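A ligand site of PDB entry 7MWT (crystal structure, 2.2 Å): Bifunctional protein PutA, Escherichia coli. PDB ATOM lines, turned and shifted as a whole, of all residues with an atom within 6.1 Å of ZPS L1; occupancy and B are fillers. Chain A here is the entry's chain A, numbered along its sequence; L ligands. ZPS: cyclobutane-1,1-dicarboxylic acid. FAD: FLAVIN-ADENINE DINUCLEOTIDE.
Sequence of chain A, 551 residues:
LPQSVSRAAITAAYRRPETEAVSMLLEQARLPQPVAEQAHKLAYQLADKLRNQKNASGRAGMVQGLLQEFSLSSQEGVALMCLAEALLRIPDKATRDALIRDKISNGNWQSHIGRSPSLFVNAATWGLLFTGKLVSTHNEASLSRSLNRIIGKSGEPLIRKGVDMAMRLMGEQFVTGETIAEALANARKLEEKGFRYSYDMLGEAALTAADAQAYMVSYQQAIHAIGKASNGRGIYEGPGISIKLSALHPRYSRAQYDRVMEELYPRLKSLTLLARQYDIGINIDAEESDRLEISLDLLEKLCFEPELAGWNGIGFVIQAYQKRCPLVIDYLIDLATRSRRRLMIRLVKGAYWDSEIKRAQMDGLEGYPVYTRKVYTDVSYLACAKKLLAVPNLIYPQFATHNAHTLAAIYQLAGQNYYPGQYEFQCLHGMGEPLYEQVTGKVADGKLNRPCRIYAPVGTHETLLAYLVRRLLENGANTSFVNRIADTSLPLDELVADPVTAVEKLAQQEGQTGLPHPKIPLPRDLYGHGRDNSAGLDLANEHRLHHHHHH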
ATOM      1  N   ASP A 200      13.892   5.306  -3.355  1.00  0.00           N
ATOM      2  CA  ASP A 200      13.263   5.060  -4.642  1.00  0.00           C
ATOM      3  C   ASP A 200      12.159   6.086  -4.832  1.00  0.00           C
ATOM      4  O   ASP A 200      11.175   6.093  -4.087  1.00  0.00           O
ATOM      5  CB  ASP A 200      12.712   3.638  -4.710  1.00  0.00           C
ATOM      6  CG  ASP A 200      11.957   3.373  -5.977  1.00  0.00           C
ATOM      7  OD1 ASP A 200      12.242   4.017  -7.014  1.00  0.00           O
ATOM      8  OD2 ASP A 200      11.059   2.497  -5.925  1.00  0.00           O
ATOM      9  N   LEU A 202       9.137   6.735  -6.521  1.00  0.00           N
ATOM     10  CA  LEU A 202       8.186   5.858  -7.199  1.00  0.00           C
ATOM     11  C   LEU A 202       7.760   6.447  -8.542  1.00  0.00           C
ATOM     12  O   LEU A 202       7.719   7.663  -8.734  1.00  0.00           O
ATOM     13  CB  LEU A 202       6.958   5.627  -6.323  1.00  0.00           C
ATOM     14  CG  LEU A 202       7.182   4.756  -5.094  1.00  0.00           C
ATOM     15  CD1 LEU A 202       5.997   4.915  -4.142  1.00  0.00           C
ATOM     16  CD2 LEU A 202       7.356   3.295  -5.497  1.00  0.00           C
ATOM     17  N   GLU A 204       7.232   4.538 -12.789  1.00  0.00           N
ATOM     18  CA  GLU A 204       7.929   3.622 -13.683  1.00  0.00           C
ATOM     19  C   GLU A 204       7.141   3.527 -14.983  1.00  0.00           C
ATOM     20  O   GLU A 204       6.009   4.025 -15.081  1.00  0.00           O
ATOM     21  CB  GLU A 204       8.102   2.247 -13.017  1.00  0.00           C
ATOM     22  CG  GLU A 204       6.770   1.461 -12.772  1.00  0.00           C
ATOM     23  CD  GLU A 204       6.986   0.216 -11.917  1.00  0.00           C
ATOM     24  OE1 GLU A 204       7.563   0.318 -10.803  1.00  0.00           O
ATOM     25  OE2 GLU A 204       6.586  -0.877 -12.353  1.00  0.00           O
ATOM     26  N   LYS A 244      14.910   3.363 -12.009  1.00  0.00           N
ATOM     27  CA  LYS A 244      14.406   2.413 -12.985  1.00  0.00           C
ATOM     28  C   LYS A 244      14.569   3.003 -14.371  1.00  0.00           C
ATOM     29  O   LYS A 244      14.082   4.113 -14.642  1.00  0.00           O
ATOM     30  CB  LYS A 244      12.953   2.037 -12.712  1.00  0.00           C
ATOM     31  CG  LYS A 244      12.790   1.109 -11.517  1.00  0.00           C
ATOM     32  CD  LYS A 244      11.322   0.820 -11.243  1.00  0.00           C
ATOM     33  CE  LYS A 244      11.145  -0.479 -10.452  1.00  0.00           C
ATOM     34  NZ  LYS A 244      11.548  -0.332  -9.026  1.00  0.00           N
ATOM     35  N   ASP A 285      17.751  -0.478 -10.800  1.00  0.00           N
ATOM     36  CA  ASP A 285      16.828  -1.583 -10.514  1.00  0.00           C
ATOM     37  C   ASP A 285      16.687  -2.473 -11.746  1.00  0.00           C
ATOM     38  O   ASP A 285      16.737  -2.010 -12.886  1.00  0.00           O
ATOM     39  CB  ASP A 285      15.456  -1.055 -10.092  1.00  0.00           C
ATOM     40  CG  ASP A 285      15.406  -0.566  -8.642  1.00  0.00           C
ATOM     41  OD1 ASP A 285      16.345  -0.799  -7.850  1.00  0.00           O
ATOM     42  OD2 ASP A 285      14.373   0.055  -8.306  1.00  0.00           O
ATOM     43  N   ALA A 286      16.508  -3.785 -11.516  1.00  0.00           N
ATOM     44  CA  ALA A 286      16.221  -4.732 -12.599  1.00  0.00           C
ATOM     45  C   ALA A 286      14.711  -4.917 -12.750  1.00  0.00           C
ATOM     46  O   ALA A 286      13.987  -5.037 -11.758  1.00  0.00           O
ATOM     47  CB  ALA A 286      16.888  -6.089 -12.331  1.00  0.00           C
ATOM     48  N   GLU A 287      14.243  -4.955 -14.007  1.00  0.00           N
ATOM     49  CA  GLU A 287      12.800  -5.016 -14.257  1.00  0.00           C
ATOM     50  C   GLU A 287      12.434  -6.281 -15.036  1.00  0.00           C
ATOM     51  O   GLU A 287      12.873  -7.374 -14.657  1.00  0.00           O
ATOM     52  CB  GLU A 287      12.335  -3.741 -14.964  1.00  0.00           C
ATOM     53  CG  GLU A 287      12.537  -2.482 -14.064  1.00  0.00           C
ATOM     54  CD  GLU A 287      12.094  -1.174 -14.719  1.00  0.00           C
ATOM     55  OE1 GLU A 287      10.885  -0.841 -14.632  1.00  0.00           O
ATOM     56  OE2 GLU A 287      12.937  -0.498 -15.339  1.00  0.00           O
ATOM     57  N   GLN A 319      18.794 -10.798 -10.941  1.00  0.00           N
ATOM     58  CA  GLN A 319      17.631 -11.558 -10.486  1.00  0.00           C
ATOM     59  C   GLN A 319      17.963 -13.042 -10.501  1.00  0.00           C
ATOM     60  O   GLN A 319      18.101 -13.648 -11.561  1.00  0.00           O
ATOM     61  CB  GLN A 319      16.408 -11.286 -11.378  1.00  0.00           C
ATOM     62  CG  GLN A 319      15.803  -9.901 -11.206  1.00  0.00           C
ATOM     63  CD  GLN A 319      15.175  -9.358 -12.484  1.00  0.00           C
ATOM     64  OE1 GLN A 319      15.634  -9.636 -13.583  1.00  0.00           O
ATOM     65  NE2 GLN A 319      14.115  -8.563 -12.333  1.00  0.00           N
ATOM     66  N   ARG A 346      23.366  -5.792  -6.230  1.00  0.00           N
ATOM     67  CA  ARG A 346      22.245  -6.321  -5.448  1.00  0.00           C
ATOM     68  C   ARG A 346      21.831  -7.650  -6.057  1.00  0.00           C
ATOM     69  O   ARG A 346      21.384  -7.704  -7.207  1.00  0.00           O
ATOM     70  CB  ARG A 346      21.052  -5.361  -5.421  1.00  0.00           C
ATOM     71  CG  ARG A 346      19.903  -5.788  -4.476  1.00  0.00           C
ATOM     72  CD  ARG A 346      18.633  -4.946  -4.662  1.00  0.00           C
ATOM     73  NE  ARG A 346      18.867  -3.528  -4.416  1.00  0.00           N
ATOM     74  CZ  ARG A 346      18.195  -2.533  -4.975  1.00  0.00           C
ATOM     75  NH1 ARG A 346      17.131  -2.748  -5.755  1.00  0.00           N
ATOM     76  NH2 ARG A 346      18.592  -1.282  -4.754  1.00  0.00           N
ATOM     77  N   GLY A 350      13.608 -11.941  -7.372  1.00  0.00           N
ATOM     78  CA  GLY A 350      12.964 -11.189  -8.436  1.00  0.00           C
ATOM     79  C   GLY A 350      11.486 -10.951  -8.156  1.00  0.00           C
ATOM     80  O   GLY A 350      10.804 -11.740  -7.507  1.00  0.00           O
ATOM     81  N   ALA A 351      10.965  -9.831  -8.690  1.00  0.00           N
ATOM     82  CA  ALA A 351       9.638  -9.359  -8.326  1.00  0.00           C
ATOM     83  C   ALA A 351       8.563  -9.582  -9.384  1.00  0.00           C
ATOM     84  O   ALA A 351       7.390  -9.343  -9.096  1.00  0.00           O
ATOM     85  CB  ALA A 351       9.703  -7.870  -7.973  1.00  0.00           C
ATOM     86  N   TYR A 352       8.918 -10.036 -10.594  1.00  0.00           N
ATOM     87  CA  TYR A 352       7.982 -10.037 -11.716  1.00  0.00           C
ATOM     88  C   TYR A 352       7.574 -11.465 -12.134  1.00  0.00           C
ATOM     89  O   TYR A 352       7.177 -11.669 -13.281  1.00  0.00           O
ATOM     90  CB  TYR A 352       8.565  -9.275 -12.910  1.00  0.00           C
ATOM     91  CG  TYR A 352       9.050  -7.863 -12.575  1.00  0.00           C
ATOM     92  CD1 TYR A 352      10.293  -7.657 -11.975  1.00  0.00           C
ATOM     93  CD2 TYR A 352       8.264  -6.743 -12.859  1.00  0.00           C
ATOM     94  CE1 TYR A 352      10.746  -6.373 -11.662  1.00  0.00           C
ATOM     95  CE2 TYR A 352       8.699  -5.466 -12.549  1.00  0.00           C
ATOM     96  CZ  TYR A 352       9.945  -5.290 -11.955  1.00  0.00           C
ATOM     97  OH  TYR A 352      10.390  -4.041 -11.636  1.00  0.00           O
ATOM     98  N   LEU A 428      13.208  -4.605   2.071  1.00  0.00           N
ATOM     99  CA  LEU A 428      12.207  -3.613   1.695  1.00  0.00           C
ATOM    100  C   LEU A 428      11.581  -2.959   2.912  1.00  0.00           C
ATOM    101  O   LEU A 428      11.257  -3.643   3.893  1.00  0.00           O
ATOM    102  CB  LEU A 428      11.082  -4.236   0.855  1.00  0.00           C
ATOM    103  CG  LEU A 428      11.458  -4.748  -0.524  1.00  0.00           C
ATOM    104  CD1 LEU A 428      10.239  -5.363  -1.284  1.00  0.00           C
ATOM    105  CD2 LEU A 428      12.097  -3.612  -1.310  1.00  0.00           C
ATOM    106  N   TYR A 455      15.406  -0.539   1.368  1.00  0.00           N
ATOM    107  CA  TYR A 455      14.875   0.083   0.159  1.00  0.00           C
ATOM    108  C   TYR A 455      13.637   0.899   0.522  1.00  0.00           C
ATOM    109  O   TYR A 455      12.660   0.373   1.051  1.00  0.00           O
ATOM    110  CB  TYR A 455      14.571  -1.006  -0.868  1.00  0.00           C
ATOM    111  CG  TYR A 455      14.219  -0.549  -2.260  1.00  0.00           C
ATOM    112  CD1 TYR A 455      12.919  -0.138  -2.566  1.00  0.00           C
ATOM    113  CD2 TYR A 455      15.166  -0.561  -3.271  1.00  0.00           C
ATOM    114  CE1 TYR A 455      12.588   0.270  -3.842  1.00  0.00           C
ATOM    115  CE2 TYR A 455      14.839  -0.135  -4.543  1.00  0.00           C
ATOM    116  CZ  TYR A 455      13.546   0.273  -4.820  1.00  0.00           C
ATOM    117  OH  TYR A 455      13.202   0.683  -6.090  1.00  0.00           O
ATOM    118  N   ALA A 466       1.941   0.155  -9.107  1.00  0.00           N
ATOM    119  CA  ALA A 466       2.705  -1.012  -9.559  1.00  0.00           C
ATOM    120  C   ALA A 466       3.525  -1.611  -8.426  1.00  0.00           C
ATOM    121  O   ALA A 466       3.592  -2.838  -8.292  1.00  0.00           O
ATOM    122  CB  ALA A 466       3.589  -0.634 -10.744  1.00  0.00           C
ATOM    123  N   TYR A 467       4.109  -0.767  -7.587  1.00  0.00           N
ATOM    124  CA  TYR A 467       4.858  -1.261  -6.425  1.00  0.00           C
ATOM    125  C   TYR A 467       3.952  -2.076  -5.506  1.00  0.00           C
ATOM    126  O   TYR A 467       4.264  -3.219  -5.164  1.00  0.00           O
ATOM    127  CB  TYR A 467       5.498  -0.088  -5.681  1.00  0.00           C
ATOM    128  CG  TYR A 467       6.541  -0.483  -4.665  1.00  0.00           C
ATOM    129  CD1 TYR A 467       6.196  -0.738  -3.344  1.00  0.00           C
ATOM    130  CD2 TYR A 467       7.877  -0.584  -5.018  1.00  0.00           C
ATOM    131  CE1 TYR A 467       7.150  -1.098  -2.403  1.00  0.00           C
ATOM    132  CE2 TYR A 467       8.847  -0.929  -4.079  1.00  0.00           C
ATOM    133  CZ  TYR A 467       8.473  -1.188  -2.769  1.00  0.00           C
ATOM    134  OH  TYR A 467       9.413  -1.536  -1.841  1.00  0.00           O
ATOM    135  N   ARG A 470       3.053  -5.526  -6.761  1.00  0.00           N
ATOM    136  CA  ARG A 470       4.177  -6.440  -6.633  1.00  0.00           C
ATOM    137  C   ARG A 470       4.360  -6.887  -5.183  1.00  0.00           C
ATOM    138  O   ARG A 470       4.747  -8.038  -4.930  1.00  0.00           O
ATOM    139  CB  ARG A 470       5.460  -5.800  -7.173  1.00  0.00           C
ATOM    140  CG  ARG A 470       5.512  -5.672  -8.708  1.00  0.00           C
ATOM    141  CD  ARG A 470       6.943  -5.367  -9.237  1.00  0.00           C
ATOM    142  NE  ARG A 470       7.411  -4.027  -8.889  1.00  0.00           N
ATOM    143  CZ  ARG A 470       7.149  -2.930  -9.583  1.00  0.00           C
ATOM    144  NH1 ARG A 470       6.378  -2.952 -10.657  1.00  0.00           N
ATOM    145  NH2 ARG A 470       7.670  -1.772  -9.173  1.00  0.00           N
ATOM    146  N   ARG A 471       4.092  -6.003  -4.218  1.00  0.00           N
ATOM    147  CA  ARG A 471       4.139  -6.394  -2.814  1.00  0.00           C
ATOM    148  C   ARG A 471       2.980  -7.313  -2.434  1.00  0.00           C
ATOM    149  O   ARG A 471       3.142  -8.223  -1.624  1.00  0.00           O
ATOM    150  CB  ARG A 471       4.169  -5.174  -1.903  1.00  0.00           C
ATOM    151  CG  ARG A 471       5.243  -4.168  -2.187  1.00  0.00           C
ATOM    152  CD  ARG A 471       6.613  -4.688  -1.780  1.00  0.00           C
ATOM    153  NE  ARG A 471       7.176  -5.609  -2.768  1.00  0.00           N
ATOM    154  CZ  ARG A 471       7.673  -5.234  -3.933  1.00  0.00           C
ATOM    155  NH1 ARG A 471       7.662  -3.972  -4.329  1.00  0.00           N
ATOM    156  NH2 ARG A 471       8.212  -6.158  -4.727  1.00  0.00           N
HETATM  157  C01 ZPS L   1      12.502  -2.866  -5.149  1.00  0.00           C
HETATM  158  C02 ZPS L   1      12.321  -2.262  -6.544  1.00  0.00           C
HETATM  159  C03 ZPS L   1      11.284  -3.349  -6.875  1.00  0.00           C
HETATM  160  C04 ZPS L   1      11.580  -4.039  -5.551  1.00  0.00           C
HETATM  161  C05 ZPS L   1      11.640  -4.202  -8.087  1.00  0.00           C
HETATM  162  C08 ZPS L   1       9.853  -2.887  -6.944  1.00  0.00           C
HETATM  163  O06 ZPS L   1      11.775  -3.657  -9.217  1.00  0.00           O
HETATM  164  O07 ZPS L   1      11.788  -5.452  -7.928  1.00  0.00           O
HETATM  165  O09 ZPS L   1       9.578  -1.774  -7.477  1.00  0.00           O
HETATM  166  O10 ZPS L   1       8.971  -3.643  -6.468  1.00  0.00           O
HETATM  167  PA  FAD L   2      11.505 -15.877  -0.711  1.00  0.00           P
HETATM  168  O1A FAD L   2      12.374 -16.953  -0.025  1.00  0.00           O
HETATM  169  O2A FAD L   2      10.092 -15.922  -0.388  1.00  0.00           O
HETATM  170  O5B FAD L   2      11.459 -15.858  -2.183  1.00  0.00           O
HETATM  171  C5B FAD L   2      10.300 -15.486  -2.933  1.00  0.00           C
HETATM  172  C4B FAD L   2      10.670 -15.350  -4.420  1.00  0.00           C
HETATM  173  O4B FAD L   2      10.824 -16.566  -5.087  1.00  0.00           O
HETATM  174  C3B FAD L   2       9.632 -14.612  -5.220  1.00  0.00           C
HETATM  175  O3B FAD L   2       9.649 -13.250  -5.036  1.00  0.00           O
HETATM  176  C2B FAD L   2      10.032 -14.964  -6.601  1.00  0.00           C
HETATM  177  O2B FAD L   2      11.184 -14.302  -6.961  1.00  0.00           O
HETATM  178  C1B FAD L   2      10.426 -16.387  -6.438  1.00  0.00           C
HETATM  179  N9A FAD L   2       9.399 -17.346  -6.808  1.00  0.00           N
HETATM  180  C8A FAD L   2       8.100 -17.423  -6.314  1.00  0.00           C
HETATM  181  N7A FAD L   2       7.469 -18.455  -6.890  1.00  0.00           N
HETATM  182  C5A FAD L   2       8.305 -19.099  -7.780  1.00  0.00           C
HETATM  183  C6A FAD L   2       8.189 -20.198  -8.617  1.00  0.00           C
HETATM  184  N6A FAD L   2       6.959 -20.957  -8.697  1.00  0.00           N
HETATM  185  N1A FAD L   2       9.232 -20.574  -9.381  1.00  0.00           N
HETATM  186  C2A FAD L   2      10.415 -19.901  -9.330  1.00  0.00           C
HETATM  187  N3A FAD L   2      10.565 -18.823  -8.516  1.00  0.00           N
HETATM  188  C4A FAD L   2       9.555 -18.394  -7.745  1.00  0.00           C
HETATM  189  N1  FAD L   2      13.375  -7.941  -7.661  1.00  0.00           N
HETATM  190  C2  FAD L   2      13.467  -7.512  -9.015  1.00  0.00           C
HETATM  191  O2  FAD L   2      12.941  -8.312  -9.969  1.00  0.00           O
HETATM  192  N3  FAD L   2      14.107  -6.315  -9.346  1.00  0.00           N
HETATM  193  C4  FAD L   2      14.652  -5.518  -8.369  1.00  0.00           C
HETATM  194  O4  FAD L   2      15.282  -4.349  -8.699  1.00  0.00           O
HETATM  195  C4X FAD L   2      14.556  -5.901  -6.919  1.00  0.00           C
HETATM  196  N5  FAD L   2      15.075  -5.115  -5.896  1.00  0.00           N
HETATM  197  C5X FAD L   2      14.937  -5.552  -4.571  1.00  0.00           C
HETATM  198  C6  FAD L   2      15.439  -4.795  -3.511  1.00  0.00           C
HETATM  199  C7  FAD L   2      15.299  -5.246  -2.203  1.00  0.00           C
HETATM  200  C7M FAD L   2      15.840  -4.406  -1.065  1.00  0.00           C
HETATM  201  C8  FAD L   2      14.657  -6.443  -1.923  1.00  0.00           C
HETATM  202  C8M FAD L   2      14.489  -6.943  -0.534  1.00  0.00           C
HETATM  203  C9  FAD L   2      14.144  -7.207  -2.970  1.00  0.00           C
HETATM  204  C9A FAD L   2      14.275  -6.760  -4.280  1.00  0.00           C
HETATM  205  N10 FAD L   2      13.745  -7.564  -5.322  1.00  0.00           N
HETATM  206  C10 FAD L   2      13.883  -7.151  -6.646  1.00  0.00           C
HETATM  207  C1' FAD L   2      13.115  -8.854  -5.016  1.00  0.00           C
HETATM  208  C2' FAD L   2      11.606  -8.881  -4.925  1.00  0.00           C
HETATM  209  O2' FAD L   2      11.085  -7.624  -4.749  1.00  0.00           O
HETATM  210  C3' FAD L   2      11.276  -9.761  -3.708  1.00  0.00           C
HETATM  211  O3' FAD L   2      11.416  -8.945  -2.607  1.00  0.00           O
HETATM  212  C4' FAD L   2      12.135 -11.010  -3.537  1.00  0.00           C
HETATM  213  O4' FAD L   2      12.134 -11.741  -4.693  1.00  0.00           O
HETATM  214  C5' FAD L   2      11.715 -11.893  -2.359  1.00  0.00           C
HETATM  215  O5' FAD L   2      12.714 -12.842  -2.011  1.00  0.00           O
HETATM  216  P   FAD L   2      12.795 -13.339  -0.488  1.00  0.00           P
HETATM  217  O1P FAD L   2      12.783 -12.217   0.631  1.00  0.00           O
HETATM  218  O2P FAD L   2      14.056 -14.269  -0.654  1.00  0.00           O
HETATM  219  O3P FAD L   2      11.583 -14.432  -0.388  1.00  0.00           O
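The guanidinium group (NH2) of Arg 470 lies within salt-bridge range of the side-chain carboxylate (OE1) of Glu 204 (2.7 Å). OH of Tyr 455 is in hydrogen-bond range of OD2 of Asp 285 (2.6 Å). OD2 of Asp 285 lies within salt-bridge range of NZ of Lys 244 (2.9 Å). The side-chain carboxylate (OD1) of Asp 285 lies within salt-bridge range of the guanidinium group (NH1) of Arg 346. The side-chain carboxylate (OD2) of Asp 200 is in hydrogen-bond range of the side-chain hydroxyl (OH) of Tyr 455 (2.8 Å).
Asp 285 touches ZPS L1. Ala 286 touches ZPS L1 (O to O06, 3.6 Å). Ala 351 touches ZPS L1. Leu 428 touches ZPS L1 (CD2 to C01, 3.9 Å). Tyr 455 touches ZPS L1 (OH to C02, 3.1 Å). Tyr 467 touches ZPS L1 (CD2 to O09, 3.2 Å). Hydrophobic or aromatic side chains that line ZPS L1: Ala 351, Tyr 352, Leu 428, Tyr 455 and Tyr 467. Ten residues have an atom within 4 Å of ZPS L1: Lys 244, Asp 285, Ala 286, Ala 351, Tyr 352, Leu 428, Tyr 455, Tyr 467, Arg 470 and Arg 471. The nearest printed residue that does not touch ZPS L1 is Glu 204 (4.4 Å).
O07 of ZPS L1 is in hydrogen-bond range of N3 of FAD L2 (2.9 Å).
N of Gly 350 is in hydrogen-bond range of O4' of FAD L2 (3.1 Å). An oxygen (O2') of FAD L2 is in hydrogen-bond range of the guanidinium group (NH2) of Arg 471, 3.2 Å away. The backbone NH of Ala 351 lies within hydrogen-bond range of an oxygen (O2) of FAD L2, at 2.8 Å. The backbone carbonyl oxygen (O) of Gly 350 lies within hydrogen-bond range of an oxygen (O2B) of FAD L2, 2.6 Å away. An oxygen (O4) of FAD L2 lies within hydrogen-bond range of the backbone NH (N) of Ala 286, 3.1 Å away. NE2 of Gln 319 lies within hydrogen-bond range of O2 of FAD L2, at 2.7 Å. The side-chain hydroxyl of Tyr 352 sits at hydrogen-bond distance from an oxygen (O06) of ZPS L1. NH1 of Arg 346 lies within hydrogen-bond range of N5 of FAD L2. O09 of ZPS L1 is in salt-bridge range of NZ of Lys 244, 2.9 Å away. The guanidinium group (NH1) of Arg 471 lies within salt-bridge range of an oxygen (O10) of ZPS L1 (2.5 Å). NH2 of Arg 470 is in salt-bridge range of O09 of ZPS L1, at 2.6 Å. O of Ala 286 lies within hydrogen-bond range of N3 of FAD L2 (2.7 Å).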
